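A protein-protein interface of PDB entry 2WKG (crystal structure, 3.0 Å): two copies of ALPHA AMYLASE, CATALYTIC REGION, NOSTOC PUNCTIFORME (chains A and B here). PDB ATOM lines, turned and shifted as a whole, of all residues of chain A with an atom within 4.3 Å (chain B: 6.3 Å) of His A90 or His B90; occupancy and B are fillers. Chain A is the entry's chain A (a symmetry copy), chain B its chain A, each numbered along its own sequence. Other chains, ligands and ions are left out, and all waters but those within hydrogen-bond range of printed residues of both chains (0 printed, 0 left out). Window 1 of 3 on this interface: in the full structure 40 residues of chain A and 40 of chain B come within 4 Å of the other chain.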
ATOM      1  N   GLN A  80      -3.986 -21.992  12.488  1.00  0.00           N
ATOM      2  CA  GLN A  80      -3.851 -22.917  11.371  1.00  0.00           C
ATOM      3  C   GLN A  80      -4.326 -22.283  10.068  1.00  0.00           C
ATOM      4  O   GLN A  80      -5.468 -21.833   9.966  1.00  0.00           O
ATOM      5  CB  GLN A  80      -4.632 -24.204  11.644  1.00  0.00           C
ATOM      6  CG  GLN A  80      -4.136 -25.410  10.862  1.00  0.00           C
ATOM      7  CD  GLN A  80      -5.056 -26.607  10.990  1.00  0.00           C
ATOM      8  OE1 GLN A  80      -6.165 -26.611  10.456  1.00  0.00           O
ATOM      9  NE2 GLN A  80      -4.600 -27.632  11.701  1.00  0.00           N
ATOM     10  N   SER A  81      -3.444 -22.251   9.075  1.00  0.00           N
ATOM     11  CA  SER A  81      -3.806 -21.780   7.743  1.00  0.00           C
ATOM     12  C   SER A  81      -2.923 -22.417   6.674  1.00  0.00           C
ATOM     13  O   SER A  81      -2.013 -23.186   6.985  1.00  0.00           O
ATOM     14  CB  SER A  81      -3.707 -20.255   7.667  1.00  0.00           C
ATOM     15  OG  SER A  81      -2.442 -19.804   8.120  1.00  0.00           O
ATOM     16  N   HIS A  88      -5.149 -16.433   5.714  1.00  0.00           N
ATOM     17  CA  HIS A  88      -6.300 -17.173   5.206  1.00  0.00           C
ATOM     18  C   HIS A  88      -6.598 -18.252   6.246  1.00  0.00           C
ATOM     19  O   HIS A  88      -6.305 -19.430   6.038  1.00  0.00           O
ATOM     20  CB  HIS A  88      -5.990 -17.836   3.858  1.00  0.00           C
ATOM     21  CG  HIS A  88      -5.457 -16.901   2.811  1.00  0.00           C
ATOM     22  ND1 HIS A  88      -5.650 -17.114   1.463  1.00  0.00           N
ATOM     23  CD2 HIS A  88      -4.695 -15.785   2.908  1.00  0.00           C
ATOM     24  CE1 HIS A  88      -5.032 -16.172   0.775  1.00  0.00           C
ATOM     25  NE2 HIS A  88      -4.443 -15.354   1.627  1.00  0.00           N
ATOM     26  N   THR A  89      -7.182 -17.842   7.368  1.00  0.00           N
ATOM     27  CA  THR A  89      -7.484 -18.754   8.462  1.00  0.00           C
ATOM     28  C   THR A  89      -8.235 -20.008   8.050  1.00  0.00           C
ATOM     29  O   THR A  89      -9.185 -19.954   7.277  1.00  0.00           O
ATOM     30  CB  THR A  89      -8.297 -18.059   9.567  1.00  0.00           C
ATOM     31  OG1 THR A  89      -7.708 -16.791   9.870  1.00  0.00           O
ATOM     32  CG2 THR A  89      -8.298 -18.908  10.833  1.00  0.00           C
ATOM     33  N   HIS A  90      -7.792 -21.141   8.584  1.00  0.00           N
ATOM     34  CA  HIS A  90      -8.417 -22.425   8.310  1.00  0.00           C
ATOM     35  C   HIS A  90      -9.173 -22.867   9.560  1.00  0.00           C
ATOM     36  O   HIS A  90     -10.291 -23.377   9.475  1.00  0.00           O
ATOM     37  CB  HIS A  90      -7.361 -23.470   7.940  1.00  0.00           C
ATOM     38  CG  HIS A  90      -7.933 -24.825   7.677  1.00  0.00           C
ATOM     39  ND1 HIS A  90      -8.348 -25.665   8.688  1.00  0.00           N
ATOM     40  CD2 HIS A  90      -8.228 -25.459   6.518  1.00  0.00           C
ATOM     41  CE1 HIS A  90      -8.878 -26.754   8.163  1.00  0.00           C
ATOM     42  NE2 HIS A  90      -8.819 -26.653   6.847  1.00  0.00           N
ATOM     43  N   ASP A  91      -8.547 -22.666  10.717  1.00  0.00           N
ATOM     44  CA  ASP A  91      -9.141 -23.013  12.004  1.00  0.00           C
ATOM     45  C   ASP A  91      -8.658 -22.049  13.081  1.00  0.00           C
ATOM     46  O   ASP A  91      -7.487 -22.055  13.460  1.00  0.00           O
ATOM     47  CB  ASP A  91      -8.767 -24.437  12.409  1.00  0.00           C
ATOM     48  CG  ASP A  91      -9.430 -24.861  13.704  1.00  0.00           C
ATOM     49  OD1 ASP A  91      -9.123 -25.961  14.206  1.00  0.00           O
ATOM     50  OD2 ASP A  91     -10.263 -24.088  14.221  1.00  0.00           O
ATOM     51  N   SER A 129     -10.928 -18.356   4.988  1.00  0.00           N
ATOM     52  CA  SER A 129     -10.315 -18.964   3.817  1.00  0.00           C
ATOM     53  C   SER A 129     -11.240 -19.993   3.205  1.00  0.00           C
ATOM     54  O   SER A 129     -12.244 -20.368   3.809  1.00  0.00           O
ATOM     55  CB  SER A 129      -9.008 -19.665   4.192  1.00  0.00           C
ATOM     56  OG  SER A 129      -9.261 -20.927   4.798  1.00  0.00           O
ATOM     57  N   GLY A 131     -10.640 -22.978   2.907  1.00  0.00           N
ATOM     58  CA  GLY A 131     -10.567 -24.122   3.800  1.00  0.00           C
ATOM     59  C   GLY A 131     -11.379 -24.038   5.078  1.00  0.00           C
ATOM     60  O   GLY A 131     -11.748 -25.069   5.635  1.00  0.00           O
ATOM     61  N   PHE A 132     -11.646 -22.825   5.557  1.00  0.00           N
ATOM     62  CA  PHE A 132     -12.429 -22.635   6.779  1.00  0.00           C
ATOM     63  C   PHE A 132     -13.667 -23.522   6.698  1.00  0.00           C
ATOM     64  O   PHE A 132     -14.432 -23.457   5.737  1.00  0.00           O
ATOM     65  CB  PHE A 132     -12.825 -21.166   6.919  1.00  0.00           C
ATOM     66  CG  PHE A 132     -13.688 -20.874   8.115  1.00  0.00           C
ATOM     67  CD1 PHE A 132     -13.216 -21.090   9.399  1.00  0.00           C
ATOM     68  CD2 PHE A 132     -14.980 -20.371   7.951  1.00  0.00           C
ATOM     69  CE1 PHE A 132     -14.019 -20.808  10.514  1.00  0.00           C
ATOM     70  CE2 PHE A 132     -15.790 -20.087   9.052  1.00  0.00           C
ATOM     71  CZ  PHE A 132     -15.310 -20.305  10.335  1.00  0.00           C
ATOM     72  N   PHE A 133     -13.857 -24.351   7.715  1.00  0.00           N
ATOM     73  CA  PHE A 133     -14.970 -25.283   7.738  1.00  0.00           C
ATOM     74  C   PHE A 133     -16.312 -24.862   7.150  1.00  0.00           C
ATOM     75  O   PHE A 133     -16.769 -25.446   6.169  1.00  0.00           O
ATOM     76  CB  PHE A 133     -15.230 -25.783   9.153  1.00  0.00           C
ATOM     77  CG  PHE A 133     -16.402 -26.717   9.234  1.00  0.00           C
ATOM     78  CD1 PHE A 133     -16.353 -27.962   8.611  1.00  0.00           C
ATOM     79  CD2 PHE A 133     -17.578 -26.332   9.875  1.00  0.00           C
ATOM     80  CE1 PHE A 133     -17.456 -28.806   8.619  1.00  0.00           C
ATOM     81  CE2 PHE A 133     -18.690 -27.171   9.889  1.00  0.00           C
ATOM     82  CZ  PHE A 133     -18.627 -28.410   9.258  1.00  0.00           C
ATOM     83  N   HIS A 136     -16.224 -24.122   3.600  1.00  0.00           N
ATOM     84  CA  HIS A 136     -16.048 -25.425   2.966  1.00  0.00           C
ATOM     85  C   HIS A 136     -17.422 -26.046   2.715  1.00  0.00           C
ATOM     86  O   HIS A 136     -17.730 -26.470   1.600  1.00  0.00           O
ATOM     87  CB  HIS A 136     -15.220 -26.333   3.883  1.00  0.00           C
ATOM     88  CG  HIS A 136     -15.243 -27.783   3.500  1.00  0.00           C
ATOM     89  ND1 HIS A 136     -14.634 -28.266   2.362  1.00  0.00           N
ATOM     90  CD2 HIS A 136     -15.808 -28.852   4.107  1.00  0.00           C
ATOM     91  CE1 HIS A 136     -14.825 -29.570   2.284  1.00  0.00           C
ATOM     92  NE2 HIS A 136     -15.535 -29.951   3.331  1.00  0.00           N
ATOM     93  N   PHE B  79     -17.361 -37.423  12.780  1.00  0.00           N
ATOM     94  CA  PHE B  79     -16.357 -36.366  12.815  1.00  0.00           C
ATOM     95  C   PHE B  79     -16.730 -35.219  11.882  1.00  0.00           C
ATOM     96  O   PHE B  79     -17.476 -35.407  10.920  1.00  0.00           O
ATOM     97  CB  PHE B  79     -14.981 -36.922  12.442  1.00  0.00           C
ATOM     98  CG  PHE B  79     -14.458 -37.943  13.411  1.00  0.00           C
ATOM     99  CD1 PHE B  79     -13.540 -38.897  13.003  1.00  0.00           C
ATOM    100  CD2 PHE B  79     -14.884 -37.951  14.728  1.00  0.00           C
ATOM    101  CE1 PHE B  79     -13.057 -39.838  13.893  1.00  0.00           C
ATOM    102  CE2 PHE B  79     -14.404 -38.890  15.622  1.00  0.00           C
ATOM    103  CZ  PHE B  79     -13.488 -39.835  15.203  1.00  0.00           C
ATOM    104  N   GLN B  80     -16.207 -34.032  12.172  1.00  0.00           N
ATOM    105  CA  GLN B  80     -16.561 -32.835  11.420  1.00  0.00           C
ATOM    106  C   GLN B  80     -16.414 -33.062   9.919  1.00  0.00           C
ATOM    107  O   GLN B  80     -15.342 -33.427   9.439  1.00  0.00           O
ATOM    108  CB  GLN B  80     -15.696 -31.651  11.859  1.00  0.00           C
ATOM    109  CG  GLN B  80     -16.317 -30.292  11.581  1.00  0.00           C
ATOM    110  CD  GLN B  80     -15.352 -29.149  11.828  1.00  0.00           C
ATOM    111  OE1 GLN B  80     -14.394 -28.959  11.080  1.00  0.00           O
ATOM    112  NE2 GLN B  80     -15.601 -28.381  12.883  1.00  0.00           N
ATOM    113  N   SER B  81     -17.500 -32.843   9.184  1.00  0.00           N
ATOM    114  CA  SER B  81     -17.464 -32.908   7.727  1.00  0.00           C
ATOM    115  C   SER B  81     -18.545 -32.026   7.110  1.00  0.00           C
ATOM    116  O   SER B  81     -19.335 -31.406   7.823  1.00  0.00           O
ATOM    117  CB  SER B  81     -17.629 -34.352   7.251  1.00  0.00           C
ATOM    118  OG  SER B  81     -18.772 -34.954   7.833  1.00  0.00           O
ATOM    119  N   ALA B  82     -18.574 -31.976   5.783  1.00  0.00           N
ATOM    120  CA  ALA B  82     -19.637 -31.283   5.066  1.00  0.00           C
ATOM    121  C   ALA B  82     -21.008 -31.648   5.625  1.00  0.00           C
ATOM    122  O   ALA B  82     -21.239 -32.784   6.039  1.00  0.00           O
ATOM    123  CB  ALA B  82     -19.568 -31.598   3.580  1.00  0.00           C
ATOM    124  N   HIS B  88     -16.793 -37.422   4.028  1.00  0.00           N
ATOM    125  CA  HIS B  88     -15.764 -36.532   3.501  1.00  0.00           C
ATOM    126  C   HIS B  88     -15.203 -35.779   4.708  1.00  0.00           C
ATOM    127  O   HIS B  88     -15.497 -34.600   4.910  1.00  0.00           O
ATOM    128  CB  HIS B  88     -16.349 -35.527   2.501  1.00  0.00           C
ATOM    129  CG  HIS B  88     -17.136 -36.147   1.384  1.00  0.00           C
ATOM    130  ND1 HIS B  88     -17.248 -35.559   0.142  1.00  0.00           N
ATOM    131  CD2 HIS B  88     -17.893 -37.270   1.333  1.00  0.00           C
ATOM    132  CE1 HIS B  88     -18.036 -36.289  -0.624  1.00  0.00           C
ATOM    133  NE2 HIS B  88     -18.443 -37.332   0.074  1.00  0.00           N
ATOM    134  N   THR B  89     -14.394 -36.469   5.506  1.00  0.00           N
ATOM    135  CA  THR B  89     -13.821 -35.891   6.714  1.00  0.00           C
ATOM    136  C   THR B  89     -13.142 -34.547   6.512  1.00  0.00           C
ATOM    137  O   THR B  89     -12.394 -34.351   5.561  1.00  0.00           O
ATOM    138  CB  THR B  89     -12.802 -36.841   7.365  1.00  0.00           C
ATOM    139  OG1 THR B  89     -13.349 -38.162   7.425  1.00  0.00           O
ATOM    140  CG2 THR B  89     -12.486 -36.383   8.783  1.00  0.00           C
ATOM    141  N   HIS B  90     -13.415 -33.626   7.429  1.00  0.00           N
ATOM    142  CA  HIS B  90     -12.827 -32.297   7.393  1.00  0.00           C
ATOM    143  C   HIS B  90     -11.793 -32.199   8.511  1.00  0.00           C
ATOM    144  O   HIS B  90     -10.707 -31.648   8.321  1.00  0.00           O
ATOM    145  CB  HIS B  90     -13.904 -31.226   7.580  1.00  0.00           C
ATOM    146  CG  HIS B  90     -13.362 -29.833   7.586  1.00  0.00           C
ATOM    147  ND1 HIS B  90     -12.701 -29.297   8.670  1.00  0.00           N
ATOM    148  CD2 HIS B  90     -13.317 -28.890   6.616  1.00  0.00           C
ATOM    149  CE1 HIS B  90     -12.269 -28.088   8.366  1.00  0.00           C
ATOM    150  NE2 HIS B  90     -12.628 -27.817   7.125  1.00  0.00           N
ATOM    151  N   ASP B  91     -12.147 -32.737   9.676  1.00  0.00           N
ATOM    152  CA  ASP B  91     -11.265 -32.746  10.838  1.00  0.00           C
ATOM    153  C   ASP B  91     -11.522 -33.990  11.681  1.00  0.00           C
ATOM    154  O   ASP B  91     -12.577 -34.129  12.301  1.00  0.00           O
ATOM    155  CB  ASP B  91     -11.490 -31.507  11.700  1.00  0.00           C
ATOM    156  CG  ASP B  91     -10.538 -31.442  12.877  1.00  0.00           C
ATOM    157  OD1 ASP B  91     -10.686 -30.538  13.724  1.00  0.00           O
ATOM    158  OD2 ASP B  91      -9.635 -32.302  12.953  1.00  0.00           O
ATOM    159  N   TYR B  92     -10.549 -34.891  11.713  1.00  0.00           N
ATOM    160  CA  TYR B  92     -10.701 -36.117  12.476  1.00  0.00           C
ATOM    161  C   TYR B  92     -10.653 -35.924  13.982  1.00  0.00           C
ATOM    162  O   TYR B  92     -11.054 -36.815  14.731  1.00  0.00           O
ATOM    163  CB  TYR B  92      -9.626 -37.135  12.087  1.00  0.00           C
ATOM    164  CG  TYR B  92      -9.775 -37.700  10.695  1.00  0.00           C
ATOM    165  CD1 TYR B  92      -9.207 -37.059   9.595  1.00  0.00           C
ATOM    166  CD2 TYR B  92     -10.487 -38.879  10.476  1.00  0.00           C
ATOM    167  CE1 TYR B  92      -9.343 -37.576   8.314  1.00  0.00           C
ATOM    168  CE2 TYR B  92     -10.628 -39.406   9.198  1.00  0.00           C
ATOM    169  CZ  TYR B  92     -10.053 -38.748   8.124  1.00  0.00           C
ATOM    170  OH  TYR B  92     -10.193 -39.262   6.862  1.00  0.00           O
ATOM    171  N   SER B 128     -10.018 -38.404   2.739  1.00  0.00           N
ATOM    172  CA  SER B 128     -10.631 -37.336   3.517  1.00  0.00           C
ATOM    173  C   SER B 128     -11.553 -36.475   2.661  1.00  0.00           C
ATOM    174  O   SER B 128     -12.513 -36.972   2.080  1.00  0.00           O
ATOM    175  CB  SER B 128      -9.551 -36.470   4.159  1.00  0.00           C
ATOM    176  OG  SER B 128      -8.644 -35.996   3.184  1.00  0.00           O
ATOM    177  N   SER B 129     -11.269 -35.183   2.582  1.00  0.00           N
ATOM    178  CA  SER B 129     -12.111 -34.291   1.799  1.00  0.00           C
ATOM    179  C   SER B 129     -11.316 -33.102   1.308  1.00  0.00           C
ATOM    180  O   SER B 129     -10.190 -32.878   1.749  1.00  0.00           O
ATOM    181  CB  SER B 129     -13.276 -33.767   2.643  1.00  0.00           C
ATOM    182  OG  SER B 129     -12.850 -32.720   3.505  1.00  0.00           O
ATOM    183  N   ARG B 130     -11.912 -32.339   0.397  1.00  0.00           N
ATOM    184  CA  ARG B 130     -11.266 -31.152  -0.137  1.00  0.00           C
ATOM    185  C   ARG B 130     -10.943 -30.237   1.048  1.00  0.00           C
ATOM    186  O   ARG B 130      -9.881 -29.619   1.098  1.00  0.00           O
ATOM    187  CB  ARG B 130     -12.212 -30.423  -1.096  1.00  0.00           C
ATOM    188  CG  ARG B 130     -12.664 -31.211  -2.317  1.00  0.00           C
ATOM    189  CD  ARG B 130     -14.139 -30.964  -2.555  1.00  0.00           C
ATOM    190  NE  ARG B 130     -14.571 -31.244  -3.920  1.00  0.00           N
ATOM    191  CZ  ARG B 130     -15.847 -31.296  -4.296  1.00  0.00           C
ATOM    192  NH1 ARG B 130     -16.812 -31.093  -3.408  1.00  0.00           N
ATOM    193  NH2 ARG B 130     -16.163 -31.533  -5.561  1.00  0.00           N
ATOM    194  N   GLY B 131     -11.869 -30.175   2.005  1.00  0.00           N
ATOM    195  CA  GLY B 131     -11.700 -29.332   3.176  1.00  0.00           C
ATOM    196  C   GLY B 131     -10.623 -29.743   4.160  1.00  0.00           C
ATOM    197  O   GLY B 131     -10.104 -28.899   4.886  1.00  0.00           O
ATOM    198  N   PHE B 132     -10.294 -31.033   4.205  1.00  0.00           N
ATOM    199  CA  PHE B 132      -9.262 -31.533   5.114  1.00  0.00           C
ATOM    200  C   PHE B 132      -8.045 -30.619   5.006  1.00  0.00           C
ATOM    201  O   PHE B 132      -7.521 -30.386   3.919  1.00  0.00           O
ATOM    202  CB  PHE B 132      -8.892 -32.969   4.742  1.00  0.00           C
ATOM    203  CG  PHE B 132      -7.791 -33.555   5.580  1.00  0.00           C
ATOM    204  CD1 PHE B 132      -7.953 -33.724   6.945  1.00  0.00           C
ATOM    205  CD2 PHE B 132      -6.587 -33.950   4.993  1.00  0.00           C
ATOM    206  CE1 PHE B 132      -6.927 -34.282   7.724  1.00  0.00           C
ATOM    207  CE2 PHE B 132      -5.558 -34.505   5.756  1.00  0.00           C
ATOM    208  CZ  PHE B 132      -5.728 -34.672   7.123  1.00  0.00           C
ATOM    209  N   PHE B 133      -7.602 -30.103   6.145  1.00  0.00           N
ATOM    210  CA  PHE B 133      -6.483 -29.179   6.177  1.00  0.00           C
ATOM    211  C   PHE B 133      -5.325 -29.373   5.206  1.00  0.00           C
ATOM    212  O   PHE B 133      -5.082 -28.522   4.351  1.00  0.00           O
ATOM    213  CB  PHE B 133      -5.892 -29.089   7.577  1.00  0.00           C
ATOM    214  CG  PHE B 133      -4.703 -28.176   7.650  1.00  0.00           C
ATOM    215  CD1 PHE B 133      -4.851 -26.809   7.429  1.00  0.00           C
ATOM    216  CD2 PHE B 133      -3.426 -28.687   7.873  1.00  0.00           C
ATOM    217  CE1 PHE B 133      -3.748 -25.965   7.423  1.00  0.00           C
ATOM    218  CE2 PHE B 133      -2.312 -27.850   7.869  1.00  0.00           C
ATOM    219  CZ  PHE B 133      -2.475 -26.486   7.644  1.00  0.00           C
ATOM    220  N   PHE B 134      -4.587 -30.466   5.343  1.00  0.00           N
ATOM    221  CA  PHE B 134      -3.433 -30.667   4.473  1.00  0.00           C
ATOM    222  C   PHE B 134      -3.759 -30.712   2.984  1.00  0.00           C
ATOM    223  O   PHE B 134      -2.959 -30.280   2.153  1.00  0.00           O
ATOM    224  CB  PHE B 134      -2.662 -31.911   4.902  1.00  0.00           C
ATOM    225  CG  PHE B 134      -2.266 -31.893   6.346  1.00  0.00           C
ATOM    226  CD1 PHE B 134      -3.122 -32.389   7.324  1.00  0.00           C
ATOM    227  CD2 PHE B 134      -1.054 -31.341   6.740  1.00  0.00           C
ATOM    228  CE1 PHE B 134      -2.775 -32.334   8.673  1.00  0.00           C
ATOM    229  CE2 PHE B 134      -0.701 -31.282   8.090  1.00  0.00           C
ATOM    230  CZ  PHE B 134      -1.562 -31.779   9.055  1.00  0.00           C
ATOM    231  N   HIS B 136      -6.239 -29.088   1.707  1.00  0.00           N
ATOM    232  CA  HIS B 136      -6.511 -27.666   1.521  1.00  0.00           C
ATOM    233  C   HIS B 136      -5.210 -26.955   1.150  1.00  0.00           C
ATOM    234  O   HIS B 136      -5.150 -26.225   0.159  1.00  0.00           O
ATOM    235  CB  HIS B 136      -7.080 -27.080   2.820  1.00  0.00           C
ATOM    236  CG  HIS B 136      -7.096 -25.581   2.864  1.00  0.00           C
ATOM    237  ND1 HIS B 136      -7.930 -24.818   2.077  1.00  0.00           N
ATOM    238  CD2 HIS B 136      -6.374 -24.708   3.603  1.00  0.00           C
ATOM    239  CE1 HIS B 136      -7.719 -23.539   2.327  1.00  0.00           C
ATOM    240  NE2 HIS B 136      -6.779 -23.445   3.250  1.00  0.00           N
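A ring nitrogen (NE2) of His B90 lies within hydrogen-bond range of the backbone carbonyl oxygen (O) of Gly A131 (3.2 Å).
The backbone carbonyl oxygen (O) of Gly B131 is in hydrogen-bond range of a ring nitrogen (NE2) of His A90 (3.2 Å).
A ring nitrogen (ND1) of His A136 lies close to the backbone NH (N) of Gly B131 (3.4 Å).
A ring nitrogen (ND1) of His B136 lies close to the backbone NH (N) of Gly A131, 3.4 Å away.
O of Gln B80 is in hydrogen-bond range of N of Asp B91 (3.3 Å).
OG of Ser B129 sits at hydrogen-bond distance from O of Thr B89.
The backbone carbonyl oxygen of Gln A80 lies within hydrogen-bond range of the backbone NH of His A90, at 2.8 Å.
The backbone carbonyl oxygen of Gln A80 sits at hydrogen-bond distance from the backbone NH of Asp A91, 3.3 Å away.
The side-chain hydroxyl (OG) of Ser A129 is in hydrogen-bond range of the backbone carbonyl oxygen (O) of Thr A89, 2.7 Å away.
The backbone NH (N) of Phe A132 lies within hydrogen-bond range of the side-chain hydroxyl (OG) of Ser A129 (3.1 Å).
Phe B133 touches Gln A80.
CE1 of His A90 touches CE1 of His B90, at 3.6 Å.
Phe B133 touches His A90 (CA to NE2, 3.5 Å).
His A90 touches His B136 (CD2 to CD2, 3.5 Å).
Ser A129 touches His B136.
Phe A133 touches Gln B80 (CD1 to OE1, 3.3 Å).
Phe A133 touches Ser B81.
Phe A133 touches His B90.
CD2 of His B90 touches CD2 of His A136 (3.5 Å).
Ser B129 touches His A136 (OG to NE2, 3.9 Å).
His A90 touches four residues of chain B.
Of the printed residues of chain A, His B90 touches His A90, Gly A131, Phe A133 and His A136.
Of the printed residues of chain B, Gly A131 touches His B90 and His B136.
Printed residues of chain B within 4 Å of Gln A80: Phe B133 (3.3 Å).
Printed residues of chain A within 4 Å of Gly B131: His A90 and His A136.
Ala B82 touches none of the printed residues of chain A.
Ser B128 touches none of the printed residues of chain A.
The nearest printed residue of chain A that does not touch His B90 is Phe A132 (4.4 Å).
Of the 11 printed residues of chain A, 7 touch a printed residue of chain B.
Printed residues of chain A that touch a printed residue of chain B: Gln A80, Ser A81, His A90, Ser A129, Gly A131, Phe A133 and His A136.
Hydrophobic or aromatic side chains of chain A within 4 Å of the printed part of chain B: His A90, Phe A133 and His A136.
Among the printed residues, 15 pairs touch across the chains.
Among the printed residues, no Asp or Glu carboxylate lies within 4 Å of a Lys or Arg side-chain nitrogen of the other chain.
Gln A80 touches Phe B133, and with the chains exchanged Phe A133 touches Gln B80.
His A90 touches its own counterpart, His B90.
His A90 touches Phe B133, and with the chains exchanged Phe A133 touches His B90.
Ser A129 touches His B136, and with the chains exchanged His A136 touches Ser B129.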
